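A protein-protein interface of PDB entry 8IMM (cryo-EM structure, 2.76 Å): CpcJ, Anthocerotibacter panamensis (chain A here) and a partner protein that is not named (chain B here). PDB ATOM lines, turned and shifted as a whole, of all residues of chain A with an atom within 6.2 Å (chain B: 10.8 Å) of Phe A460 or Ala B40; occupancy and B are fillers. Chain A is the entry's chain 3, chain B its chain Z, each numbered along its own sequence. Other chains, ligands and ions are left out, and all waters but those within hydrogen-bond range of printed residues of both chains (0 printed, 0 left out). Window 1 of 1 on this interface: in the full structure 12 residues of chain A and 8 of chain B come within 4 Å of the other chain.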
ATOM      1  N   LEU A 422      15.368 -10.868  -4.465  1.00  0.00           N
ATOM      2  CA  LEU A 422      16.362  -9.910  -4.021  1.00  0.00           C
ATOM      3  C   LEU A 422      17.067 -10.339  -2.751  1.00  0.00           C
ATOM      4  O   LEU A 422      18.130  -9.804  -2.446  1.00  0.00           O
ATOM      5  CB  LEU A 422      15.717  -8.545  -3.799  1.00  0.00           C
ATOM      6  CG  LEU A 422      14.955  -7.939  -4.965  1.00  0.00           C
ATOM      7  CD1 LEU A 422      14.186  -6.774  -4.474  1.00  0.00           C
ATOM      8  CD2 LEU A 422      15.890  -7.511  -6.045  1.00  0.00           C
ATOM      9  N   GLU A 455      18.629  -2.687 -10.472  1.00  0.00           N
ATOM     10  CA  GLU A 455      20.035  -2.418 -10.209  1.00  0.00           C
ATOM     11  C   GLU A 455      20.519  -3.160  -8.980  1.00  0.00           C
ATOM     12  O   GLU A 455      21.695  -3.513  -8.890  1.00  0.00           O
ATOM     13  CB  GLU A 455      20.250  -0.920 -10.042  1.00  0.00           C
ATOM     14  CG  GLU A 455      20.020  -0.125 -11.309  1.00  0.00           C
ATOM     15  CD  GLU A 455      18.557   0.182 -11.551  1.00  0.00           C
ATOM     16  OE1 GLU A 455      17.719  -0.175 -10.694  1.00  0.00           O
ATOM     17  OE2 GLU A 455      18.244   0.775 -12.604  1.00  0.00           O
ATOM     18  N   GLU A 456      19.632  -3.399  -8.023  1.00  0.00           N
ATOM     19  CA  GLU A 456      19.985  -4.167  -6.837  1.00  0.00           C
ATOM     20  C   GLU A 456      20.381  -5.591  -7.200  1.00  0.00           C
ATOM     21  O   GLU A 456      21.442  -6.084  -6.789  1.00  0.00           O
ATOM     22  CB  GLU A 456      18.795  -4.153  -5.885  1.00  0.00           C
ATOM     23  CG  GLU A 456      18.894  -5.050  -4.705  1.00  0.00           C
ATOM     24  CD  GLU A 456      18.272  -4.423  -3.494  1.00  0.00           C
ATOM     25  OE1 GLU A 456      18.886  -4.490  -2.410  1.00  0.00           O
ATOM     26  OE2 GLU A 456      17.186  -3.830  -3.632  1.00  0.00           O
ATOM     27  N   TYR A 457      19.537  -6.262  -7.981  1.00  0.00           N
ATOM     28  CA  TYR A 457      19.825  -7.622  -8.411  1.00  0.00           C
ATOM     29  C   TYR A 457      21.156  -7.693  -9.136  1.00  0.00           C
ATOM     30  O   TYR A 457      21.994  -8.547  -8.834  1.00  0.00           O
ATOM     31  CB  TYR A 457      18.697  -8.118  -9.315  1.00  0.00           C
ATOM     32  CG  TYR A 457      18.762  -9.583  -9.661  1.00  0.00           C
ATOM     33  CD1 TYR A 457      19.658 -10.056 -10.594  1.00  0.00           C
ATOM     34  CD2 TYR A 457      17.932 -10.493  -9.041  1.00  0.00           C
ATOM     35  CE1 TYR A 457      19.724 -11.374 -10.894  1.00  0.00           C
ATOM     36  CE2 TYR A 457      17.989 -11.814  -9.347  1.00  0.00           C
ATOM     37  CZ  TYR A 457      18.891 -12.252 -10.265  1.00  0.00           C
ATOM     38  OH  TYR A 457      18.957 -13.582 -10.579  1.00  0.00           O
ATOM     39  N   LEU A 458      21.371  -6.798 -10.092  1.00  0.00           N
ATOM     40  CA  LEU A 458      22.590  -6.833 -10.882  1.00  0.00           C
ATOM     41  C   LEU A 458      23.815  -6.496 -10.054  1.00  0.00           C
ATOM     42  O   LEU A 458      24.886  -7.065 -10.279  1.00  0.00           O
ATOM     43  CB  LEU A 458      22.453  -5.883 -12.050  1.00  0.00           C
ATOM     44  CG  LEU A 458      21.377  -6.376 -12.990  1.00  0.00           C
ATOM     45  CD1 LEU A 458      20.837  -5.219 -13.733  1.00  0.00           C
ATOM     46  CD2 LEU A 458      22.006  -7.350 -13.932  1.00  0.00           C
ATOM     47  N   ASP A 459      23.685  -5.582  -9.098  1.00  0.00           N
ATOM     48  CA  ASP A 459      24.799  -5.307  -8.211  1.00  0.00           C
ATOM     49  C   ASP A 459      25.182  -6.528  -7.400  1.00  0.00           C
ATOM     50  O   ASP A 459      26.368  -6.831  -7.277  1.00  0.00           O
ATOM     51  CB  ASP A 459      24.467  -4.147  -7.282  1.00  0.00           C
ATOM     52  CG  ASP A 459      24.374  -2.833  -8.007  1.00  0.00           C
ATOM     53  OD1 ASP A 459      25.062  -2.673  -9.036  1.00  0.00           O
ATOM     54  OD2 ASP A 459      23.622  -1.950  -7.547  1.00  0.00           O
ATOM     55  N   PHE A 460      24.212  -7.253  -6.861  1.00  0.00           N
ATOM     56  CA  PHE A 460      24.570  -8.300  -5.916  1.00  0.00           C
ATOM     57  C   PHE A 460      24.675  -9.678  -6.540  1.00  0.00           C
ATOM     58  O   PHE A 460      25.519 -10.471  -6.125  1.00  0.00           O
ATOM     59  CB  PHE A 460      23.567  -8.335  -4.773  1.00  0.00           C
ATOM     60  CG  PHE A 460      23.676  -7.162  -3.863  1.00  0.00           C
ATOM     61  CD1 PHE A 460      24.537  -7.178  -2.791  1.00  0.00           C
ATOM     62  CD2 PHE A 460      22.914  -6.036  -4.084  1.00  0.00           C
ATOM     63  CE1 PHE A 460      24.633  -6.105  -1.967  1.00  0.00           C
ATOM     64  CE2 PHE A 460      23.005  -4.965  -3.259  1.00  0.00           C
ATOM     65  CZ  PHE A 460      23.868  -4.999  -2.195  1.00  0.00           C
ATOM     66  N   PHE A 461      23.840  -9.990  -7.519  1.00  0.00           N
ATOM     67  CA  PHE A 461      23.851 -11.304  -8.137  1.00  0.00           C
ATOM     68  C   PHE A 461      24.416 -11.297  -9.546  1.00  0.00           C
ATOM     69  O   PHE A 461      25.229 -12.154  -9.876  1.00  0.00           O
ATOM     70  CB  PHE A 461      22.441 -11.891  -8.134  1.00  0.00           C
ATOM     71  CG  PHE A 461      21.774 -11.818  -6.802  1.00  0.00           C
ATOM     72  CD1 PHE A 461      22.448 -12.170  -5.664  1.00  0.00           C
ATOM     73  CD2 PHE A 461      20.485 -11.371  -6.683  1.00  0.00           C
ATOM     74  CE1 PHE A 461      21.843 -12.079  -4.446  1.00  0.00           C
ATOM     75  CE2 PHE A 461      19.890 -11.280  -5.469  1.00  0.00           C
ATOM     76  CZ  PHE A 461      20.566 -11.642  -4.352  1.00  0.00           C
ATOM     77  N   GLY A 462      24.014 -10.344 -10.375  1.00  0.00           N
ATOM     78  CA  GLY A 462      24.666 -10.078 -11.638  1.00  0.00           C
ATOM     79  C   GLY A 462      24.915 -11.233 -12.581  1.00  0.00           C
ATOM     80  O   GLY A 462      26.065 -11.634 -12.783  1.00  0.00           O
ATOM     81  N   THR A 465      25.496 -15.390 -10.418  1.00  0.00           N
ATOM     82  CA  THR A 465      25.372 -15.971  -9.094  1.00  0.00           C
ATOM     83  C   THR A 465      23.910 -16.163  -8.747  1.00  0.00           C
ATOM     84  O   THR A 465      23.058 -15.348  -9.102  1.00  0.00           O
ATOM     85  CB  THR A 465      26.049 -15.115  -8.027  1.00  0.00           C
ATOM     86  OG1 THR A 465      25.465 -13.817  -8.016  1.00  0.00           O
ATOM     87  CG2 THR A 465      27.524 -14.990  -8.310  1.00  0.00           C
ATOM     88  N   TYR A 468      20.768 -15.072  -2.986  1.00  0.00           N
ATOM     89  CA  TYR A 468      20.912 -15.556  -1.629  1.00  0.00           C
ATOM     90  C   TYR A 468      20.286 -14.533  -0.698  1.00  0.00           C
ATOM     91  O   TYR A 468      19.959 -13.419  -1.102  1.00  0.00           O
ATOM     92  CB  TYR A 468      22.379 -15.800  -1.266  1.00  0.00           C
ATOM     93  CG  TYR A 468      23.277 -14.613  -1.483  1.00  0.00           C
ATOM     94  CD1 TYR A 468      23.785 -14.327  -2.731  1.00  0.00           C
ATOM     95  CD2 TYR A 468      23.633 -13.791  -0.437  1.00  0.00           C
ATOM     96  CE1 TYR A 468      24.586 -13.258  -2.935  1.00  0.00           C
ATOM     97  CE2 TYR A 468      24.442 -12.718  -0.636  1.00  0.00           C
ATOM     98  CZ  TYR A 468      24.920 -12.458  -1.885  1.00  0.00           C
ATOM     99  OH  TYR A 468      25.739 -11.381  -2.096  1.00  0.00           O
ATOM    100  N   ARG A 470      20.421 -11.744   1.529  1.00  0.00           N
ATOM    101  CA  ARG A 470      21.323 -10.666   1.897  1.00  0.00           C
ATOM    102  C   ARG A 470      20.948 -10.000   3.204  1.00  0.00           C
ATOM    103  O   ARG A 470      21.825  -9.717   4.022  1.00  0.00           O
ATOM    104  CB  ARG A 470      21.344  -9.602   0.810  1.00  0.00           C
ATOM    105  CG  ARG A 470      22.012 -10.032  -0.415  1.00  0.00           C
ATOM    106  CD  ARG A 470      21.971  -8.955  -1.425  1.00  0.00           C
ATOM    107  NE  ARG A 470      20.630  -8.484  -1.704  1.00  0.00           N
ATOM    108  CZ  ARG A 470      20.241  -7.229  -1.557  1.00  0.00           C
ATOM    109  NH1 ARG A 470      21.080  -6.318  -1.110  1.00  0.00           N
ATOM    110  NH2 ARG A 470      19.004  -6.891  -1.854  1.00  0.00           N
ATOM    111  N   GLN A 475      22.516  -3.752   4.799  1.00  0.00           N
ATOM    112  CA  GLN A 475      22.629  -3.351   3.408  1.00  0.00           C
ATOM    113  C   GLN A 475      22.490  -1.841   3.339  1.00  0.00           C
ATOM    114  O   GLN A 475      21.691  -1.258   4.070  1.00  0.00           O
ATOM    115  CB  GLN A 475      21.541  -4.002   2.550  1.00  0.00           C
ATOM    116  CG  GLN A 475      21.448  -5.521   2.576  1.00  0.00           C
ATOM    117  CD  GLN A 475      22.724  -6.215   2.188  1.00  0.00           C
ATOM    118  OE1 GLN A 475      23.351  -5.864   1.203  1.00  0.00           O
ATOM    119  NE2 GLN A 475      23.086  -7.244   2.933  1.00  0.00           N
ATOM    120  N   THR A 476      23.270  -1.198   2.483  1.00  0.00           N
ATOM    121  CA  THR A 476      23.211   0.254   2.413  1.00  0.00           C
ATOM    122  C   THR A 476      21.859   0.689   1.873  1.00  0.00           C
ATOM    123  O   THR A 476      21.375   0.143   0.880  1.00  0.00           O
ATOM    124  CB  THR A 476      24.330   0.801   1.538  1.00  0.00           C
ATOM    125  OG1 THR A 476      24.267   0.186   0.251  1.00  0.00           O
ATOM    126  CG2 THR A 476      25.665   0.476   2.158  1.00  0.00           C
ATOM    127  N   TYR B  29      33.045   0.544 -17.306  1.00  0.00           N
ATOM    128  CA  TYR B  29      32.666  -0.508 -16.375  1.00  0.00           C
ATOM    129  C   TYR B  29      33.789  -0.787 -15.392  1.00  0.00           C
ATOM    130  O   TYR B  29      33.541  -1.029 -14.204  1.00  0.00           O
ATOM    131  CB  TYR B  29      32.316  -1.772 -17.149  1.00  0.00           C
ATOM    132  CG  TYR B  29      31.464  -2.763 -16.399  1.00  0.00           C
ATOM    133  CD1 TYR B  29      30.081  -2.707 -16.472  1.00  0.00           C
ATOM    134  CD2 TYR B  29      32.042  -3.768 -15.637  1.00  0.00           C
ATOM    135  CE1 TYR B  29      29.294  -3.615 -15.798  1.00  0.00           C
ATOM    136  CE2 TYR B  29      31.264  -4.680 -14.957  1.00  0.00           C
ATOM    137  CZ  TYR B  29      29.889  -4.600 -15.044  1.00  0.00           C
ATOM    138  OH  TYR B  29      29.107  -5.507 -14.368  1.00  0.00           O
ATOM    139  N   ASN B  32      33.846   1.975 -12.789  1.00  0.00           N
ATOM    140  CA  ASN B  32      32.683   1.841 -11.918  1.00  0.00           C
ATOM    141  C   ASN B  32      32.882   0.719 -10.907  1.00  0.00           C
ATOM    142  O   ASN B  32      32.570   0.876  -9.719  1.00  0.00           O
ATOM    143  CB  ASN B  32      31.425   1.601 -12.748  1.00  0.00           C
ATOM    144  CG  ASN B  32      30.920   2.863 -13.413  1.00  0.00           C
ATOM    145  OD1 ASN B  32      31.570   3.907 -13.365  1.00  0.00           O
ATOM    146  ND2 ASN B  32      29.754   2.775 -14.042  1.00  0.00           N
ATOM    147  N   LYS B  33      33.414  -0.419 -11.358  1.00  0.00           N
ATOM    148  CA  LYS B  33      33.714  -1.515 -10.442  1.00  0.00           C
ATOM    149  C   LYS B  33      34.825  -1.145  -9.471  1.00  0.00           C
ATOM    150  O   LYS B  33      34.808  -1.583  -8.316  1.00  0.00           O
ATOM    151  CB  LYS B  33      34.099  -2.767 -11.225  1.00  0.00           C
ATOM    152  CG  LYS B  33      32.936  -3.670 -11.589  1.00  0.00           C
ATOM    153  CD  LYS B  33      32.283  -4.279 -10.357  1.00  0.00           C
ATOM    154  CE  LYS B  33      31.143  -5.202 -10.752  1.00  0.00           C
ATOM    155  NZ  LYS B  33      30.086  -4.478 -11.500  1.00  0.00           N
ATOM    156  N   HIS B  34      35.803  -0.359  -9.923  1.00  0.00           N
ATOM    157  CA  HIS B  34      36.861   0.105  -9.032  1.00  0.00           C
ATOM    158  C   HIS B  34      36.310   0.988  -7.922  1.00  0.00           C
ATOM    159  O   HIS B  34      36.737   0.866  -6.768  1.00  0.00           O
ATOM    160  CB  HIS B  34      37.924   0.859  -9.828  1.00  0.00           C
ATOM    161  CG  HIS B  34      38.680   0.001 -10.794  1.00  0.00           C
ATOM    162  ND1 HIS B  34      39.187   0.488 -11.978  1.00  0.00           N
ATOM    163  CD2 HIS B  34      39.029  -1.305 -10.745  1.00  0.00           C
ATOM    164  CE1 HIS B  34      39.807  -0.483 -12.624  1.00  0.00           C
ATOM    165  NE2 HIS B  34      39.726  -1.583 -11.897  1.00  0.00           N
ATOM    166  N   THR B  36      33.031   1.060  -6.825  1.00  0.00           N
ATOM    167  CA  THR B  36      32.089   0.334  -5.985  1.00  0.00           C
ATOM    168  C   THR B  36      32.740  -0.866  -5.309  1.00  0.00           C
ATOM    169  O   THR B  36      32.315  -1.273  -4.223  1.00  0.00           O
ATOM    170  CB  THR B  36      30.880  -0.097  -6.813  1.00  0.00           C
ATOM    171  OG1 THR B  36      30.488   0.982  -7.668  1.00  0.00           O
ATOM    172  CG2 THR B  36      29.715  -0.448  -5.903  1.00  0.00           C
ATOM    173  N   GLY B  37      33.763  -1.440  -5.925  1.00  0.00           N
ATOM    174  CA  GLY B  37      34.405  -2.620  -5.393  1.00  0.00           C
ATOM    175  C   GLY B  37      33.792  -3.893  -5.948  1.00  0.00           C
ATOM    176  O   GLY B  37      32.614  -3.947  -6.312  1.00  0.00           O
ATOM    177  N   TYR B  38      34.606  -4.942  -6.019  1.00  0.00           N
ATOM    178  CA  TYR B  38      34.145  -6.202  -6.581  1.00  0.00           C
ATOM    179  C   TYR B  38      33.191  -6.869  -5.608  1.00  0.00           C
ATOM    180  O   TYR B  38      33.523  -7.108  -4.443  1.00  0.00           O
ATOM    181  CB  TYR B  38      35.298  -7.119  -6.967  1.00  0.00           C
ATOM    182  CG  TYR B  38      35.635  -6.898  -8.413  1.00  0.00           C
ATOM    183  CD1 TYR B  38      34.650  -7.016  -9.384  1.00  0.00           C
ATOM    184  CD2 TYR B  38      36.907  -6.535  -8.810  1.00  0.00           C
ATOM    185  CE1 TYR B  38      34.923  -6.802 -10.707  1.00  0.00           C
ATOM    186  CE2 TYR B  38      37.190  -6.319 -10.138  1.00  0.00           C
ATOM    187  CZ  TYR B  38      36.195  -6.453 -11.081  1.00  0.00           C
ATOM    188  OH  TYR B  38      36.471  -6.241 -12.406  1.00  0.00           O
ATOM    189  N   ARG B  39      32.010  -7.166  -6.117  1.00  0.00           N
ATOM    190  CA  ARG B  39      30.794  -7.228  -5.336  1.00  0.00           C
ATOM    191  C   ARG B  39      29.958  -8.434  -5.722  1.00  0.00           C
ATOM    192  O   ARG B  39      29.133  -8.887  -4.925  1.00  0.00           O
ATOM    193  CB  ARG B  39      30.080  -5.892  -5.577  1.00  0.00           C
ATOM    194  CG  ARG B  39      28.617  -5.649  -5.435  1.00  0.00           C
ATOM    195  CD  ARG B  39      28.266  -5.358  -3.996  1.00  0.00           C
ATOM    196  NE  ARG B  39      26.882  -4.919  -3.903  1.00  0.00           N
ATOM    197  CZ  ARG B  39      26.488  -3.730  -4.367  1.00  0.00           C
ATOM    198  NH1 ARG B  39      27.370  -2.901  -4.910  1.00  0.00           N
ATOM    199  NH2 ARG B  39      25.230  -3.341  -4.276  1.00  0.00           N
ATOM    200  N   ALA B  40      30.168  -8.961  -6.923  1.00  0.00           N
ATOM    201  CA  ALA B  40      29.966 -10.327  -7.366  1.00  0.00           C
ATOM    202  C   ALA B  40      31.278 -10.743  -8.018  1.00  0.00           C
ATOM    203  O   ALA B  40      32.054  -9.876  -8.434  1.00  0.00           O
ATOM    204  CB  ALA B  40      28.800 -10.449  -8.362  1.00  0.00           C
ATOM    205  N   PRO B  41      31.565 -12.044  -8.104  1.00  0.00           N
ATOM    206  CA  PRO B  41      32.884 -12.475  -8.596  1.00  0.00           C
ATOM    207  C   PRO B  41      33.208 -11.932  -9.983  1.00  0.00           C
ATOM    208  O   PRO B  41      32.329 -11.737 -10.824  1.00  0.00           O
ATOM    209  CB  PRO B  41      32.778 -14.006  -8.606  1.00  0.00           C
ATOM    210  CG  PRO B  41      31.319 -14.303  -8.447  1.00  0.00           C
ATOM    211  CD  PRO B  41      30.766 -13.185  -7.641  1.00  0.00           C
ATOM    212  N   ILE B  42      34.500 -11.668 -10.196  1.00  0.00           N
ATOM    213  CA  ILE B  42      34.967 -11.037 -11.426  1.00  0.00           C
ATOM    214  C   ILE B  42      34.736 -11.954 -12.624  1.00  0.00           C
ATOM    215  O   ILE B  42      34.750 -13.186 -12.509  1.00  0.00           O
ATOM    216  CB  ILE B  42      36.452 -10.657 -11.290  1.00  0.00           C
ATOM    217  CG1 ILE B  42      36.914  -9.835 -12.492  1.00  0.00           C
ATOM    218  CG2 ILE B  42      37.312 -11.900 -11.122  1.00  0.00           C
ATOM    219  CD1 ILE B  42      38.316  -9.323 -12.375  1.00  0.00           C
ATOM    220  N   ARG B  43      34.511 -11.347 -13.789  1.00  0.00           N
ATOM    221  CA  ARG B  43      34.241 -12.085 -15.014  1.00  0.00           C
ATOM    222  C   ARG B  43      34.953 -11.422 -16.185  1.00  0.00           C
ATOM    223  O   ARG B  43      35.404 -10.279 -16.100  1.00  0.00           O
ATOM    224  CB  ARG B  43      32.736 -12.174 -15.284  1.00  0.00           C
ATOM    225  CG  ARG B  43      32.074 -10.833 -15.541  1.00  0.00           C
ATOM    226  CD  ARG B  43      30.636 -11.012 -16.012  1.00  0.00           C
ATOM    227  NE  ARG B  43      29.894 -11.901 -15.124  1.00  0.00           N
ATOM    228  CZ  ARG B  43      28.912 -11.501 -14.321  1.00  0.00           C
ATOM    229  NH1 ARG B  43      28.543 -10.228 -14.300  1.00  0.00           N
ATOM    230  NH2 ARG B  43      28.293 -12.375 -13.541  1.00  0.00           N
ATOM    231  N   GLN B  44      35.059 -12.164 -17.284  1.00  0.00           N
ATOM    232  CA  GLN B  44      35.723 -11.648 -18.472  1.00  0.00           C
ATOM    233  C   GLN B  44      34.887 -10.560 -19.132  1.00  0.00           C
ATOM    234  O   GLN B  44      33.674 -10.471 -18.937  1.00  0.00           O
ATOM    235  CB  GLN B  44      36.005 -12.774 -19.464  1.00  0.00           C
ATOM    236  CG  GLN B  44      36.541 -14.030 -18.822  1.00  0.00           C
ATOM    237  CD  GLN B  44      38.022 -13.946 -18.535  1.00  0.00           C
ATOM    238  OE1 GLN B  44      38.615 -12.873 -18.593  1.00  0.00           O
ATOM    239  NE2 GLN B  44      38.626 -15.079 -18.212  1.00  0.00           N
ATOM    240  N   ARG B  62      20.333  -0.223 -19.933  1.00  0.00           N
ATOM    241  CA  ARG B  62      21.072  -0.732 -18.787  1.00  0.00           C
ATOM    242  C   ARG B  62      22.547  -0.899 -19.111  1.00  0.00           C
ATOM    243  O   ARG B  62      23.413  -0.547 -18.303  1.00  0.00           O
ATOM    244  CB  ARG B  62      20.466  -2.059 -18.359  1.00  0.00           C
ATOM    245  CG  ARG B  62      20.901  -2.552 -17.021  1.00  0.00           C
ATOM    246  CD  ARG B  62      20.331  -3.932 -16.796  1.00  0.00           C
ATOM    247  NE  ARG B  62      20.840  -4.926 -17.736  1.00  0.00           N
ATOM    248  CZ  ARG B  62      22.068  -5.428 -17.703  1.00  0.00           C
ATOM    249  NH1 ARG B  62      22.927  -5.025 -16.781  1.00  0.00           N
ATOM    250  NH2 ARG B  62      22.438  -6.336 -18.591  1.00  0.00           N
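Of chain B, only Arg B39 and Ala B40 come within 4 Å of Phe A460.
Of chain A, only Phe A460 (3.97 Å) comes within 4 Å of Ala B40.
No residue of chain B comes within 4 Å of Glu A456.
Gly A462 touches one residue of chain B.
Printed residues of chain B within 4 Å of Thr A465: Pro B41 (3.8 Å).
Printed residues of chain B within 4 Å of Leu A458: Arg B62 (3.4 Å).
Of the printed residues of chain A, Arg B39 touches Asp A459 (3.1 Å) and Phe A460 (2.9 Å).
Of the printed residues of chain A, Pro B41 touches Thr A465 (3.8 Å).
Printed residues of chain A within 4 Å of Arg B43: Gly A462 (2.5 Å).
Printed residues of chain A within 4 Å of Arg B62: Leu A458 (3.4 Å).
Tyr A468 touches none of the printed residues of chain B.
Lys B33 touches none of the printed residues of chain A.
The nearest residue of chain B that does not touch Phe A460 is Pro B41 (6.1 Å).
The nearest residue of chain A that does not touch Ala B40 is Phe A461 (4.2 Å).
The nearest printed residue of chain A that does not touch Arg B39 is Tyr A468 (5.1 Å).
Arg B62 touches Leu A458.
Phe A460 touches Arg B39 (CE2 to NH2, 2.9 Å).
CB of Ala B40 touches O of Phe A460 (3.97 Å).
Thr A465 touches Pro B41 (CG2 to CD, 3.8 Å).
Hydrophobic or aromatic side chains of chain B within 4 Å of the printed part of chain A: Ala B40 and Pro B41.
Of the 14 printed residues of chain A, 5 touch a printed residue of chain B.
Among the printed residues, 6 pairs touch across the chains.
Among the printed residues, Asp or Glu carboxylates within 4 Å of a Lys or Arg side-chain nitrogen of the other chain: Asp A459 with Arg B39 (3.9 Å).
OD2 of Asp A459 lies within salt-bridge range of NH2 of Arg B39 (3.9 Å).
O of Gly A462 is in hydrogen-bond range of NH2 of Arg B43, at 2.5 Å.
O of Phe A461 lies within hydrogen-bond range of OG1 of Thr A465 (2.5 Å).
O of Tyr A457 sits at hydrogen-bond distance from N of Gly A462 (3.1 Å).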
